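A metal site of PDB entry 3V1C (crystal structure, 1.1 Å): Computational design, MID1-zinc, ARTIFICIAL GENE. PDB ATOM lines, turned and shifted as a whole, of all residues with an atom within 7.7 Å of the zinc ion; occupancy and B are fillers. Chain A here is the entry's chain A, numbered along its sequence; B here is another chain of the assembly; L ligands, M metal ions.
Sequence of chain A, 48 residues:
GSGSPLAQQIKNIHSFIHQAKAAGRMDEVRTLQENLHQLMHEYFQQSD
The backbone carbonyl oxygen of His 41 of chain B lies close to the side-chain amide oxygen of Gln 45 of chain B (2.9 Å).
Along chain A the residues within 4 Å of the zinc ion span positions 14 to 18.
The zinc ion is bound by an oxygen (O6) of the ligand (2.0 Å), a ring nitrogen (ND1) of His 41 of chain B (2.0 Å), a ring nitrogen (NE2) of His 18 (2.0 Å) and a ring nitrogen (NE2) of His 14 (2.0 Å). The zinc ion has four donor atoms within binding distance.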
ATOM      1  N   HIS A  14      -5.588  15.360 -14.274  1.00  0.00           N
ATOM      2  CA  HIS A  14      -5.986  14.044 -13.836  1.00  0.00           C
ATOM      3  C   HIS A  14      -5.060  13.553 -12.718  1.00  0.00           C
ATOM      4  O   HIS A  14      -5.531  13.032 -11.703  1.00  0.00           O
ATOM      5  CB  HIS A  14      -5.964  13.075 -15.010  1.00  0.00           C
ATOM      6  CG  HIS A  14      -6.265  11.677 -14.607  1.00  0.00           C
ATOM      7  ND1 HIS A  14      -5.288  10.726 -14.424  1.00  0.00           N
ATOM      8  CD2 HIS A  14      -7.435  11.083 -14.284  1.00  0.00           C
ATOM      9  CE1 HIS A  14      -5.846   9.599 -14.024  1.00  0.00           C
ATOM     10  NE2 HIS A  14      -7.149   9.795 -13.920  1.00  0.00           N
ATOM     11  N   SER A  15      -3.749  13.745 -12.864  1.00  0.00           N
ATOM     12  CA  SER A  15      -2.809  13.407 -11.800  1.00  0.00           C
ATOM     13  C   SER A  15      -3.127  14.161 -10.526  1.00  0.00           C
ATOM     14  O   SER A  15      -3.119  13.603  -9.435  1.00  0.00           O
ATOM     15  CB  SER A  15      -1.365  13.694 -12.244  1.00  0.00           C
ATOM     16  OG  SER A  15      -0.975  12.854 -13.316  1.00  0.00           O
ATOM     17  N   ILE A  17      -5.984  15.342  -9.573  1.00  0.00           N
ATOM     18  CA  ILE A  17      -7.201  14.798  -8.974  1.00  0.00           C
ATOM     19  C   ILE A  17      -6.846  13.644  -8.047  1.00  0.00           C
ATOM     20  O   ILE A  17      -7.343  13.563  -6.920  1.00  0.00           O
ATOM     21  CB  ILE A  17      -8.207  14.351 -10.055  1.00  0.00           C
ATOM     22  CG1 ILE A  17      -8.853  15.581 -10.699  1.00  0.00           C
ATOM     23  CG2 ILE A  17      -9.270  13.442  -9.441  1.00  0.00           C
ATOM     24  CD1 ILE A  17      -9.609  15.308 -11.963  1.00  0.00           C
ATOM     25  N   HIS A  18      -6.004  12.724  -8.513  1.00  0.00           N
ATOM     26  CA  HIS A  18      -5.660  11.576  -7.689  1.00  0.00           C
ATOM     27  C   HIS A  18      -4.814  11.949  -6.489  1.00  0.00           C
ATOM     28  O   HIS A  18      -4.963  11.366  -5.412  1.00  0.00           O
ATOM     29  CB  HIS A  18      -5.037  10.480  -8.535  1.00  0.00           C
ATOM     30  CG  HIS A  18      -6.061   9.800  -9.361  1.00  0.00           C
ATOM     31  ND1 HIS A  18      -7.052   9.024  -8.808  1.00  0.00           N
ATOM     32  CD2 HIS A  18      -6.370   9.916 -10.671  1.00  0.00           C
ATOM     33  CE1 HIS A  18      -7.878   8.627  -9.758  1.00  0.00           C
ATOM     34  NE2 HIS A  18      -7.475   9.143 -10.904  1.00  0.00           N
ATOM     35  N   LYS A  21      -7.385  13.315  -4.055  1.00  0.00           N
ATOM     36  CA  LYS A  21      -8.159  12.223  -3.436  1.00  0.00           C
ATOM     37  C   LYS A  21      -7.348  11.522  -2.343  1.00  0.00           C
ATOM     38  O   LYS A  21      -7.874  11.215  -1.270  1.00  0.00           O
ATOM     39  CB  LYS A  21      -8.589  11.207  -4.483  1.00  0.00           C
ATOM     40  CG  LYS A  21      -9.679  11.674  -5.420  1.00  0.00           C
ATOM     41  CD  LYS A  21     -10.006  10.598  -6.445  1.00  0.00           C
ATOM     42  CE  LYS A  21     -11.217  10.893  -7.252  1.00  0.00           C
ATOM     43  NZ  LYS A  21     -11.459   9.738  -8.169  1.00  0.00           N
ATOM     44  N   LEU A  36     -11.336  19.616 -15.451  1.00  0.00           N
ATOM     45  CA  LEU A  36     -11.005  18.513 -16.344  1.00  0.00           C
ATOM     46  C   LEU A  36     -12.116  18.272 -17.365  1.00  0.00           C
ATOM     47  O   LEU A  36     -11.836  18.106 -18.560  1.00  0.00           O
ATOM     48  CB  LEU A  36     -10.778  17.241 -15.523  1.00  0.00           C
ATOM     49  CG  LEU A  36     -10.488  15.981 -16.341  1.00  0.00           C
ATOM     50  CD1 LEU A  36      -9.271  16.203 -17.208  1.00  0.00           C
ATOM     51  CD2 LEU A  36     -10.326  14.746 -15.456  1.00  0.00           C
ATOM     52  N   HIS B  37     -15.597   8.839 -18.212  1.00  0.00           N
ATOM     53  CA  HIS B  37     -14.668   9.127 -17.148  1.00  0.00           C
ATOM     54  C   HIS B  37     -13.760   7.944 -16.874  1.00  0.00           C
ATOM     55  O   HIS B  37     -12.589   8.124 -16.566  1.00  0.00           O
ATOM     56  CB  HIS B  37     -15.410   9.550 -15.881  1.00  0.00           C
ATOM     57  CG  HIS B  37     -16.232  10.788 -16.065  1.00  0.00           C
ATOM     58  ND1 HIS B  37     -17.273  11.111 -15.234  1.00  0.00           N
ATOM     59  CD2 HIS B  37     -16.190  11.742 -17.015  1.00  0.00           C
ATOM     60  CE1 HIS B  37     -17.838  12.233 -15.651  1.00  0.00           C
ATOM     61  NE2 HIS B  37     -17.195  12.637 -16.736  1.00  0.00           N
ATOM     62  N   GLN B  38     -14.300   6.733 -16.978  1.00  0.00           N
ATOM     63  CA  GLN B  38     -13.500   5.540 -16.793  1.00  0.00           C
ATOM     64  C   GLN B  38     -12.442   5.380 -17.895  1.00  0.00           C
ATOM     65  O   GLN B  38     -11.293   5.039 -17.608  1.00  0.00           O
ATOM     66  CB  GLN B  38     -14.411   4.311 -16.757  1.00  0.00           C
ATOM     67  CG  GLN B  38     -13.669   3.027 -16.450  1.00  0.00           C
ATOM     68  CD  GLN B  38     -13.103   2.995 -15.037  1.00  0.00           C
ATOM     69  OE1 GLN B  38     -13.478   3.780 -14.179  1.00  0.00           O
ATOM     70  NE2 GLN B  38     -12.234   2.019 -14.797  1.00  0.00           N
ATOM     71  N   MET B  40     -11.142   7.764 -19.705  1.00  0.00           N
ATOM     72  CA  MET B  40     -10.124   8.787 -19.483  1.00  0.00           C
ATOM     73  C   MET B  40      -9.215   8.407 -18.317  1.00  0.00           C
ATOM     74  O   MET B  40      -7.997   8.629 -18.387  1.00  0.00           O
ATOM     75  CB  MET B  40     -10.762  10.143 -19.214  1.00  0.00           C
ATOM     76  CG  MET B  40     -11.657  10.605 -20.336  1.00  0.00           C
ATOM     77  SD  MET B  40     -11.091  12.070 -21.166  1.00  0.00           S
ATOM     78  CE  MET B  40     -12.678  12.871 -21.392  1.00  0.00           C
ATOM     79  N   HIS B  41      -9.775   7.851 -17.252  1.00  0.00           N
ATOM     80  CA  HIS B  41      -8.974   7.427 -16.127  1.00  0.00           C
ATOM     81  C   HIS B  41      -7.904   6.428 -16.569  1.00  0.00           C
ATOM     82  O   HIS B  41      -6.755   6.500 -16.126  1.00  0.00           O
ATOM     83  CB  HIS B  41      -9.901   6.834 -15.060  1.00  0.00           C
ATOM     84  CG  HIS B  41      -9.187   6.168 -13.934  1.00  0.00           C
ATOM     85  ND1 HIS B  41      -8.542   6.846 -12.919  1.00  0.00           N
ATOM     86  CD2 HIS B  41      -9.018   4.852 -13.665  1.00  0.00           C
ATOM     87  CE1 HIS B  41      -8.011   5.982 -12.086  1.00  0.00           C
ATOM     88  NE2 HIS B  41      -8.285   4.769 -12.509  1.00  0.00           N
ATOM     89  N   GLU B  42      -8.264   5.477 -17.416  1.00  0.00           N
ATOM     90  CA  GLU B  42      -7.271   4.525 -17.877  1.00  0.00           C
ATOM     91  C   GLU B  42      -6.293   5.185 -18.887  1.00  0.00           C
ATOM     92  O   GLU B  42      -5.092   4.957 -18.799  1.00  0.00           O
ATOM     93  CB  GLU B  42      -7.927   3.263 -18.440  1.00  0.00           C
ATOM     94  CG  GLU B  42      -8.807   2.506 -17.431  1.00  0.00           C
ATOM     95  CD  GLU B  42      -8.102   2.100 -16.135  1.00  0.00           C
ATOM     96  OE1 GLU B  42      -6.863   2.075 -16.080  1.00  0.00           O
ATOM     97  OE2 GLU B  42      -8.812   1.838 -15.141  1.00  0.00           O
ATOM     98  N   PHE B  44      -5.171   8.155 -19.071  1.00  0.00           N
ATOM     99  CA  PHE B  44      -4.232   9.092 -18.483  1.00  0.00           C
ATOM    100  C   PHE B  44      -3.370   8.471 -17.378  1.00  0.00           C
ATOM    101  O   PHE B  44      -2.638   9.191 -16.700  1.00  0.00           O
ATOM    102  CB  PHE B  44      -4.963  10.385 -18.046  1.00  0.00           C
ATOM    103  CG  PHE B  44      -5.394  11.247 -19.227  1.00  0.00           C
ATOM    104  CD1 PHE B  44      -4.447  11.864 -20.033  1.00  0.00           C
ATOM    105  CD2 PHE B  44      -6.737  11.392 -19.562  1.00  0.00           C
ATOM    106  CE1 PHE B  44      -4.828  12.644 -21.106  1.00  0.00           C
ATOM    107  CE2 PHE B  44      -7.114  12.176 -20.656  1.00  0.00           C
ATOM    108  CZ  PHE B  44      -6.158  12.795 -21.431  1.00  0.00           C
ATOM    109  N   GLN B  45      -3.417   7.150 -17.228  1.00  0.00           N
ATOM    110  CA  GLN B  45      -2.437   6.419 -16.397  1.00  0.00           C
ATOM    111  C   GLN B  45      -1.032   6.531 -16.998  1.00  0.00           C
ATOM    112  O   GLN B  45      -0.860   6.899 -18.162  1.00  0.00           O
ATOM    113  CB  GLN B  45      -2.759   4.917 -16.309  1.00  0.00           C
ATOM    114  CG  GLN B  45      -4.114   4.532 -15.783  1.00  0.00           C
ATOM    115  CD  GLN B  45      -4.261   4.792 -14.314  1.00  0.00           C
ATOM    116  OE1 GLN B  45      -5.068   5.655 -13.917  1.00  0.00           O
ATOM    117  NE2 GLN B  45      -3.505   4.063 -13.481  1.00  0.00           N
HETATM  118  O1  LIG L   1     -14.960  11.682 -12.986  1.00  0.00           O
HETATM  119  O2  LIG L   1     -13.453  12.980 -13.963  1.00  0.00           O
HETATM  120  C1  LIG L   1     -13.811  11.926 -13.387  1.00  0.00           C
HETATM  121  C2  LIG L   1     -12.754  10.886 -13.104  1.00  0.00           C
HETATM  122  O3  LIG L   1     -13.365   9.673 -12.594  1.00  0.00           O
HETATM  123  C3  LIG L   1     -11.669  11.270 -12.124  1.00  0.00           C
HETATM  124  O4  LIG L   1     -12.263  11.689 -10.888  1.00  0.00           O
HETATM  125  C4  LIG L   1     -10.622  10.228 -11.973  1.00  0.00           C
HETATM  126  O5  LIG L   1     -10.502   9.653 -10.850  1.00  0.00           O
HETATM  127  O6  LIG L   1      -9.967   9.924 -13.009  1.00  0.00           O
HETATM  128 ZN    ZN M   1      -8.400   8.817 -12.656  1.00  0.00          ZN
